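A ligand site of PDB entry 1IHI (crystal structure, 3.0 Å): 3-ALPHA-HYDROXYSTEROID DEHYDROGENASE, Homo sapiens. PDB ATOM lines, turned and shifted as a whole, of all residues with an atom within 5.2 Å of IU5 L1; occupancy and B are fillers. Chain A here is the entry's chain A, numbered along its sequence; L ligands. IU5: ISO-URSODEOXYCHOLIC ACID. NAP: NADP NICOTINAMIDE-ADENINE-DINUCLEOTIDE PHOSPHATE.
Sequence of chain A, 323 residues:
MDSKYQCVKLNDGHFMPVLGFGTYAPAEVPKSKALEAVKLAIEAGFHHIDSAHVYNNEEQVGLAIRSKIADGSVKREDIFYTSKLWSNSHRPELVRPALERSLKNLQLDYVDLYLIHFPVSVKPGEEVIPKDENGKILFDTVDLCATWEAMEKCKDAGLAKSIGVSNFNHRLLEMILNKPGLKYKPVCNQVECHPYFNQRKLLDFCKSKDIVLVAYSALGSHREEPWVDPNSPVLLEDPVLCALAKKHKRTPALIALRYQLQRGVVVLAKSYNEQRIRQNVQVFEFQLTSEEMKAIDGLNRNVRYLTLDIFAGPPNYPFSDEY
An oxygen (O4A) of IU5 L1 sits at hydrogen-bond distance from the side-chain hydroxyl (OH) of Tyr 55 (2.7 Å). A ring nitrogen (NE2) of His 117 is in hydrogen-bond range of an oxygen (O4A) of IU5 L1 (2.7 Å). The side-chain hydroxyl (OH) of Tyr 24 is in hydrogen-bond range of an oxygen (O1A) of IU5 L1 (2.8 Å). N7N of NAP L2 lies within hydrogen-bond range of NE2 of His 117 (3.4 Å). The backbone NH of Tyr 24 lies within hydrogen-bond range of an oxygen (O3D) of NAP L2 (3.1 Å).
NZ of Lys 84 lies within hydrogen-bond range of OH of Tyr 55, 3.1 Å away. The side-chain hydroxyl (OH) of Tyr 24 sits at hydrogen-bond distance from the side-chain carboxylate (OE1) of Glu 224, at 2.5 Å. O of Val 128 lies within hydrogen-bond range of NE1 of Trp 86 (2.6 Å).
Residues that only touch IU5 L1: Val 54 (3.5 Å), Trp 86 (3.3 Å), Val 128 (3.9 Å), Ile 129 (3.8 Å), Glu 224 (3.7 Å), Trp 227 (3.9 Å) and Leu 308 (3.9 Å). Along chain A the residues within 4 Å of IU5 L1 span positions 24 to 308.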
ATOM      1  N   TYR A  24       2.126  19.343 -23.950  1.00  0.00           N
ATOM      2  CA  TYR A  24       1.255  19.923 -22.923  1.00  0.00           C
ATOM      3  C   TYR A  24       1.678  21.323 -22.510  1.00  0.00           C
ATOM      4  O   TYR A  24       2.860  21.656 -22.531  1.00  0.00           O
ATOM      5  CB  TYR A  24       1.228  19.051 -21.666  1.00  0.00           C
ATOM      6  CG  TYR A  24       0.566  19.771 -20.501  1.00  0.00           C
ATOM      7  CD1 TYR A  24      -0.805  19.948 -20.454  1.00  0.00           C
ATOM      8  CD2 TYR A  24       1.331  20.335 -19.481  1.00  0.00           C
ATOM      9  CE1 TYR A  24      -1.406  20.683 -19.440  1.00  0.00           C
ATOM     10  CE2 TYR A  24       0.747  21.070 -18.468  1.00  0.00           C
ATOM     11  CZ  TYR A  24      -0.618  21.247 -18.450  1.00  0.00           C
ATOM     12  OH  TYR A  24      -1.202  21.990 -17.464  1.00  0.00           O
ATOM     13  N   PRO A  26       0.034  24.876 -19.880  1.00  0.00           N
ATOM     14  CA  PRO A  26      -1.020  25.375 -18.988  1.00  0.00           C
ATOM     15  C   PRO A  26      -2.148  26.055 -19.776  1.00  0.00           C
ATOM     16  O   PRO A  26      -1.919  26.560 -20.881  1.00  0.00           O
ATOM     17  CB  PRO A  26      -0.280  26.364 -18.101  1.00  0.00           C
ATOM     18  CG  PRO A  26       1.125  25.813 -18.075  1.00  0.00           C
ATOM     19  CD  PRO A  26       1.336  25.454 -19.513  1.00  0.00           C
ATOM     20  N   ALA A  27      -3.345  26.062 -19.207  1.00  0.00           N
ATOM     21  CA  ALA A  27      -4.493  26.678 -19.872  1.00  0.00           C
ATOM     22  C   ALA A  27      -4.264  28.170 -20.135  1.00  0.00           C
ATOM     23  O   ALA A  27      -4.852  28.754 -21.048  1.00  0.00           O
ATOM     24  CB  ALA A  27      -5.736  26.466 -19.040  1.00  0.00           C
ATOM     25  N   VAL A  54      -6.220  14.224 -22.055  1.00  0.00           N
ATOM     26  CA  VAL A  54      -6.264  15.210 -20.962  1.00  0.00           C
ATOM     27  C   VAL A  54      -5.531  16.503 -21.318  1.00  0.00           C
ATOM     28  O   VAL A  54      -5.760  17.528 -20.687  1.00  0.00           O
ATOM     29  CB  VAL A  54      -5.635  14.694 -19.627  1.00  0.00           C
ATOM     30  CG1 VAL A  54      -6.721  14.176 -18.706  1.00  0.00           C
ATOM     31  CG2 VAL A  54      -4.597  13.604 -19.889  1.00  0.00           C
ATOM     32  N   TYR A  55      -4.660  16.465 -22.315  1.00  0.00           N
ATOM     33  CA  TYR A  55      -3.946  17.671 -22.695  1.00  0.00           C
ATOM     34  C   TYR A  55      -4.882  18.613 -23.407  1.00  0.00           C
ATOM     35  O   TYR A  55      -4.605  19.799 -23.564  1.00  0.00           O
ATOM     36  CB  TYR A  55      -2.754  17.332 -23.582  1.00  0.00           C
ATOM     37  CG  TYR A  55      -1.703  16.550 -22.835  1.00  0.00           C
ATOM     38  CD1 TYR A  55      -0.578  16.051 -23.487  1.00  0.00           C
ATOM     39  CD2 TYR A  55      -1.836  16.295 -21.465  1.00  0.00           C
ATOM     40  CE1 TYR A  55       0.373  15.309 -22.793  1.00  0.00           C
ATOM     41  CE2 TYR A  55      -0.898  15.568 -20.767  1.00  0.00           C
ATOM     42  CZ  TYR A  55       0.210  15.072 -21.432  1.00  0.00           C
ATOM     43  OH  TYR A  55       1.137  14.341 -20.750  1.00  0.00           O
ATOM     44  N   LYS A  84      -2.579   9.040 -25.005  1.00  0.00           N
ATOM     45  CA  LYS A  84      -2.709   8.268 -23.792  1.00  0.00           C
ATOM     46  C   LYS A  84      -4.157   8.158 -23.374  1.00  0.00           C
ATOM     47  O   LYS A  84      -4.921   9.117 -23.491  1.00  0.00           O
ATOM     48  CB  LYS A  84      -1.878   8.938 -22.686  1.00  0.00           C
ATOM     49  CG  LYS A  84      -0.530   9.482 -23.158  1.00  0.00           C
ATOM     50  CD  LYS A  84       0.359   9.879 -21.989  1.00  0.00           C
ATOM     51  CE  LYS A  84       1.617  10.622 -22.441  1.00  0.00           C
ATOM     52  NZ  LYS A  84       1.345  12.065 -22.780  1.00  0.00           N
ATOM     53  N   TRP A  86      -7.099   8.157 -20.850  1.00  0.00           N
ATOM     54  CA  TRP A  86      -7.272   8.810 -19.553  1.00  0.00           C
ATOM     55  C   TRP A  86      -8.084   7.998 -18.542  1.00  0.00           C
ATOM     56  O   TRP A  86      -9.028   7.300 -18.868  1.00  0.00           O
ATOM     57  CB  TRP A  86      -7.899  10.200 -19.693  1.00  0.00           C
ATOM     58  CG  TRP A  86      -7.953  10.915 -18.374  1.00  0.00           C
ATOM     59  CD1 TRP A  86      -9.066  11.376 -17.733  1.00  0.00           C
ATOM     60  CD2 TRP A  86      -6.848  11.178 -17.503  1.00  0.00           C
ATOM     61  NE1 TRP A  86      -8.726  11.912 -16.522  1.00  0.00           N
ATOM     62  CE2 TRP A  86      -7.373  11.800 -16.346  1.00  0.00           C
ATOM     63  CE3 TRP A  86      -5.469  10.949 -17.579  1.00  0.00           C
ATOM     64  CZ2 TRP A  86      -6.560  12.193 -15.286  1.00  0.00           C
ATOM     65  CZ3 TRP A  86      -4.667  11.335 -16.521  1.00  0.00           C
ATOM     66  CH2 TRP A  86      -5.216  11.957 -15.386  1.00  0.00           C
ATOM     67  N   HIS A 117      -2.525   6.230 -19.353  1.00  0.00           N
ATOM     68  CA  HIS A 117      -1.941   7.412 -18.740  1.00  0.00           C
ATOM     69  C   HIS A 117      -1.567   7.336 -17.272  1.00  0.00           C
ATOM     70  O   HIS A 117      -0.444   7.652 -16.900  1.00  0.00           O
ATOM     71  CB  HIS A 117      -2.861   8.606 -18.965  1.00  0.00           C
ATOM     72  CG  HIS A 117      -2.142   9.919 -18.934  1.00  0.00           C
ATOM     73  ND1 HIS A 117      -2.536  10.986 -19.711  1.00  0.00           N
ATOM     74  CD2 HIS A 117      -1.050  10.320 -18.260  1.00  0.00           C
ATOM     75  CE1 HIS A 117      -1.705  11.998 -19.509  1.00  0.00           C
ATOM     76  NE2 HIS A 117      -0.785  11.611 -18.629  1.00  0.00           N
ATOM     77  N   VAL A 128     -12.919  15.201 -16.648  1.00  0.00           N
ATOM     78  CA  VAL A 128     -11.673  14.442 -16.662  1.00  0.00           C
ATOM     79  C   VAL A 128     -11.224  14.086 -15.243  1.00  0.00           C
ATOM     80  O   VAL A 128     -10.549  13.087 -15.011  1.00  0.00           O
ATOM     81  CB  VAL A 128     -10.593  15.260 -17.413  1.00  0.00           C
ATOM     82  CG1 VAL A 128      -9.233  15.075 -16.787  1.00  0.00           C
ATOM     83  CG2 VAL A 128     -10.546  14.822 -18.847  1.00  0.00           C
ATOM     84  N   ILE A 129     -11.610  14.928 -14.278  1.00  0.00           N
ATOM     85  CA  ILE A 129     -11.293  14.684 -12.885  1.00  0.00           C
ATOM     86  C   ILE A 129     -12.565  15.000 -12.097  1.00  0.00           C
ATOM     87  O   ILE A 129     -12.699  16.089 -11.517  1.00  0.00           O
ATOM     88  CB  ILE A 129     -10.101  15.567 -12.424  1.00  0.00           C
ATOM     89  CG1 ILE A 129      -8.840  15.113 -13.176  1.00  0.00           C
ATOM     90  CG2 ILE A 129      -9.898  15.439 -10.931  1.00  0.00           C
ATOM     91  CD1 ILE A 129      -7.558  15.773 -12.691  1.00  0.00           C
ATOM     92  N   GLU A 224       4.079  23.831 -13.032  1.00  0.00           N
ATOM     93  CA  GLU A 224       2.808  24.544 -12.884  1.00  0.00           C
ATOM     94  C   GLU A 224       2.399  24.537 -11.411  1.00  0.00           C
ATOM     95  O   GLU A 224       2.328  23.483 -10.782  1.00  0.00           O
ATOM     96  CB  GLU A 224       1.713  23.895 -13.751  1.00  0.00           C
ATOM     97  CG  GLU A 224       0.666  24.896 -14.247  1.00  0.00           C
ATOM     98  CD  GLU A 224      -0.272  24.309 -15.299  1.00  0.00           C
ATOM     99  OE1 GLU A 224       0.204  23.549 -16.163  1.00  0.00           O
ATOM    100  OE2 GLU A 224      -1.475  24.623 -15.262  1.00  0.00           O
ATOM    101  N   TRP A 227       0.253  21.719  -9.559  1.00  0.00           N
ATOM    102  CA  TRP A 227       0.890  20.419  -9.746  1.00  0.00           C
ATOM    103  C   TRP A 227       2.319  20.223  -9.257  1.00  0.00           C
ATOM    104  O   TRP A 227       2.682  19.119  -8.841  1.00  0.00           O
ATOM    105  CB  TRP A 227       0.784  20.043 -11.226  1.00  0.00           C
ATOM    106  CG  TRP A 227      -0.588  20.260 -11.725  1.00  0.00           C
ATOM    107  CD1 TRP A 227      -1.056  21.343 -12.401  1.00  0.00           C
ATOM    108  CD2 TRP A 227      -1.717  19.428 -11.469  1.00  0.00           C
ATOM    109  NE1 TRP A 227      -2.411  21.243 -12.577  1.00  0.00           N
ATOM    110  CE2 TRP A 227      -2.842  20.068 -12.018  1.00  0.00           C
ATOM    111  CE3 TRP A 227      -1.884  18.200 -10.820  1.00  0.00           C
ATOM    112  CZ2 TRP A 227      -4.118  19.525 -11.943  1.00  0.00           C
ATOM    113  CZ3 TRP A 227      -3.150  17.665 -10.743  1.00  0.00           C
ATOM    114  CH2 TRP A 227      -4.252  18.326 -11.302  1.00  0.00           C
ATOM    115  N   LEU A 306       6.379  15.773 -10.195  1.00  0.00           N
ATOM    116  CA  LEU A 306       4.946  15.481 -10.283  1.00  0.00           C
ATOM    117  C   LEU A 306       4.577  14.282  -9.431  1.00  0.00           C
ATOM    118  O   LEU A 306       4.872  13.140  -9.795  1.00  0.00           O
ATOM    119  CB  LEU A 306       4.540  15.223 -11.731  1.00  0.00           C
ATOM    120  CG  LEU A 306       4.311  16.483 -12.584  1.00  0.00           C
ATOM    121  CD1 LEU A 306       4.519  16.187 -14.063  1.00  0.00           C
ATOM    122  CD2 LEU A 306       2.921  17.029 -12.325  1.00  0.00           C
ATOM    123  N   LEU A 308       1.345  14.015  -8.324  1.00  0.00           N
ATOM    124  CA  LEU A 308      -0.076  13.810  -8.586  1.00  0.00           C
ATOM    125  C   LEU A 308      -0.720  13.159  -7.351  1.00  0.00           C
ATOM    126  O   LEU A 308      -1.442  12.176  -7.488  1.00  0.00           O
ATOM    127  CB  LEU A 308      -0.272  12.887  -9.789  1.00  0.00           C
ATOM    128  CG  LEU A 308       0.588  13.050 -11.052  1.00  0.00           C
ATOM    129  CD1 LEU A 308       0.058  12.114 -12.135  1.00  0.00           C
ATOM    130  CD2 LEU A 308       0.563  14.485 -11.545  1.00  0.00           C
ATOM    131  N   PHE A 311      -4.427  11.971  -6.274  1.00  0.00           N
ATOM    132  CA  PHE A 311      -4.921  10.627  -6.574  1.00  0.00           C
ATOM    133  C   PHE A 311      -4.294   9.667  -5.567  1.00  0.00           C
ATOM    134  O   PHE A 311      -4.308   8.467  -5.765  1.00  0.00           O
ATOM    135  CB  PHE A 311      -4.505  10.203  -7.990  1.00  0.00           C
ATOM    136  CG  PHE A 311      -4.970  11.133  -9.082  1.00  0.00           C
ATOM    137  CD1 PHE A 311      -4.069  11.953  -9.741  1.00  0.00           C
ATOM    138  CD2 PHE A 311      -6.316  11.175  -9.446  1.00  0.00           C
ATOM    139  CE1 PHE A 311      -4.496  12.815 -10.764  1.00  0.00           C
ATOM    140  CE2 PHE A 311      -6.754  12.025 -10.458  1.00  0.00           C
ATOM    141  CZ  PHE A 311      -5.847  12.851 -11.123  1.00  0.00           C
HETATM  142  C1  IU5 L   1      -9.040  19.597 -15.468  1.00  0.00           C
HETATM  143  C10 IU5 L   1      -7.702  20.071 -16.128  1.00  0.00           C
HETATM  144  C11 IU5 L   1      -6.526  17.736 -15.972  1.00  0.00           C
HETATM  145  C12 IU5 L   1      -5.262  16.935 -15.477  1.00  0.00           C
HETATM  146  C13 IU5 L   1      -3.960  17.424 -16.154  1.00  0.00           C
HETATM  147  C14 IU5 L   1      -3.866  18.948 -15.767  1.00  0.00           C
HETATM  148  C15 IU5 L   1      -2.444  19.368 -16.282  1.00  0.00           C
HETATM  149  C16 IU5 L   1      -1.612  18.070 -16.076  1.00  0.00           C
HETATM  150  C17 IU5 L   1      -2.601  16.982 -15.504  1.00  0.00           C
HETATM  151  C18 IU5 L   1      -3.970  17.204 -17.725  1.00  0.00           C
HETATM  152  C19 IU5 L   1      -7.908  19.978 -17.683  1.00  0.00           C
HETATM  153  O1A IU5 L   1      -3.815  21.942 -16.442  1.00  0.00           O
HETATM  154  O1B IU5 L   1      -8.774  21.347 -12.089  1.00  0.00           O
HETATM  155  C2  IU5 L   1      -9.036  19.684 -13.904  1.00  0.00           C
HETATM  156  C20 IU5 L   1      -2.072  15.505 -15.788  1.00  0.00           C
HETATM  157  C21 IU5 L   1      -2.986  14.426 -15.310  1.00  0.00           C
HETATM  158  C22 IU5 L   1      -0.652  15.413 -15.182  1.00  0.00           C
HETATM  159  C23 IU5 L   1       0.260  14.592 -15.991  1.00  0.00           C
HETATM  160  C24 IU5 L   1       0.428  14.961 -17.521  1.00  0.00           C
HETATM  161  C3  IU5 L   1      -8.814  21.186 -13.540  1.00  0.00           C
HETATM  162  C4  IU5 L   1      -7.497  21.738 -14.120  1.00  0.00           C
HETATM  163  O4  IU5 L   1       0.558  16.157 -17.892  1.00  0.00           O
HETATM  164  O4A IU5 L   1       0.436  13.957 -18.200  1.00  0.00           O
HETATM  165  C5  IU5 L   1      -7.545  21.601 -15.675  1.00  0.00           C
HETATM  166  C6  IU5 L   1      -6.233  22.148 -16.299  1.00  0.00           C
HETATM  167  C7  IU5 L   1      -5.003  21.333 -15.851  1.00  0.00           C
HETATM  168  C8  IU5 L   1      -5.116  19.829 -16.269  1.00  0.00           C
HETATM  169  C9  IU5 L   1      -6.420  19.243 -15.626  1.00  0.00           C
HETATM  170  PA  NAP L   2       9.982  19.614 -19.731  1.00  0.00           P
HETATM  171  O1A NAP L   2      11.029  19.373 -18.733  1.00  0.00           O
HETATM  172  O2A NAP L   2       9.922  18.873 -20.960  1.00  0.00           O
HETATM  173  O5B NAP L   2       9.962  21.226 -20.050  1.00  0.00           O
HETATM  174  C5B NAP L   2       9.619  22.285 -18.990  1.00  0.00           C
HETATM  175  C4B NAP L   2      10.053  23.503 -19.640  1.00  0.00           C
HETATM  176  O4B NAP L   2      11.557  23.519 -20.032  1.00  0.00           O
HETATM  177  C3B NAP L   2       9.408  23.896 -20.685  1.00  0.00           C
HETATM  178  O3B NAP L   2       8.238  24.566 -20.381  1.00  0.00           O
HETATM  179  C2B NAP L   2      10.299  24.799 -21.525  1.00  0.00           C
HETATM  180  O2B NAP L   2       9.956  26.056 -21.555  1.00  0.00           O
HETATM  181  C1B NAP L   2      11.661  24.530 -21.055  1.00  0.00           C
HETATM  182  N9A NAP L   2      12.599  24.117 -22.156  1.00  0.00           N
HETATM  183  C8A NAP L   2      12.541  23.249 -23.259  1.00  0.00           C
HETATM  184  N7A NAP L   2      13.658  23.200 -23.947  1.00  0.00           N
HETATM  185  C5A NAP L   2      14.505  24.067 -23.294  1.00  0.00           C
HETATM  186  C6A NAP L   2      15.867  24.472 -23.518  1.00  0.00           C
HETATM  187  N6A NAP L   2      16.571  24.005 -24.534  1.00  0.00           N
HETATM  188  N1A NAP L   2      16.447  25.401 -22.637  1.00  0.00           N
HETATM  189  C2A NAP L   2      15.730  25.900 -21.583  1.00  0.00           C
HETATM  190  N3A NAP L   2      14.446  25.556 -21.307  1.00  0.00           N
HETATM  191  C4A NAP L   2      13.883  24.631 -22.202  1.00  0.00           C
HETATM  192  O3  NAP L   2       8.744  19.276 -18.764  1.00  0.00           O
HETATM  193  PN  NAP L   2       7.171  18.856 -18.980  1.00  0.00           P
HETATM  194  O1N NAP L   2       6.367  20.033 -18.647  1.00  0.00           O
HETATM  195  O2N NAP L   2       7.016  17.665 -18.108  1.00  0.00           O
HETATM  196  O5D NAP L   2       6.868  18.365 -20.472  1.00  0.00           O
HETATM  197  C5D NAP L   2       7.495  17.226 -21.106  1.00  0.00           C
HETATM  198  C4D NAP L   2       6.443  16.393 -21.849  1.00  0.00           C
HETATM  199  O4D NAP L   2       6.308  15.103 -21.218  1.00  0.00           O
HETATM  200  C3D NAP L   2       4.987  16.945 -21.837  1.00  0.00           C
HETATM  201  O3D NAP L   2       4.685  17.982 -22.800  1.00  0.00           O
HETATM  202  C2D NAP L   2       4.147  15.728 -22.036  1.00  0.00           C
HETATM  203  O2D NAP L   2       3.872  15.401 -23.382  1.00  0.00           O
HETATM  204  C1D NAP L   2       4.963  14.638 -21.281  1.00  0.00           C
HETATM  205  N1N NAP L   2       4.427  14.329 -19.932  1.00  0.00           N
HETATM  206  C2N NAP L   2       3.808  13.049 -19.714  1.00  0.00           C
HETATM  207  C3N NAP L   2       3.321  12.807 -18.370  1.00  0.00           C
HETATM  208  C7N NAP L   2       2.661  11.557 -18.003  1.00  0.00           C
HETATM  209  O7N NAP L   2       2.241  11.347 -16.857  1.00  0.00           O
HETATM  210  N7N NAP L   2       2.482  10.574 -18.907  1.00  0.00           N
HETATM  211  C4N NAP L   2       3.489  13.820 -17.376  1.00  0.00           C
HETATM  212  C5N NAP L   2       4.070  15.032 -17.598  1.00  0.00           C
HETATM  213  C6N NAP L   2       4.551  15.286 -18.865  1.00  0.00           C
HETATM  214  P2B NAP L   2       9.462  26.636 -23.006  1.00  0.00           P
HETATM  215  O1X NAP L   2       8.296  25.823 -23.506  1.00  0.00           O
HETATM  216  O2X NAP L   2       9.157  28.016 -22.680  1.00  0.00           O
HETATM  217  O3X NAP L   2      10.650  26.519 -23.855  1.00  0.00           O
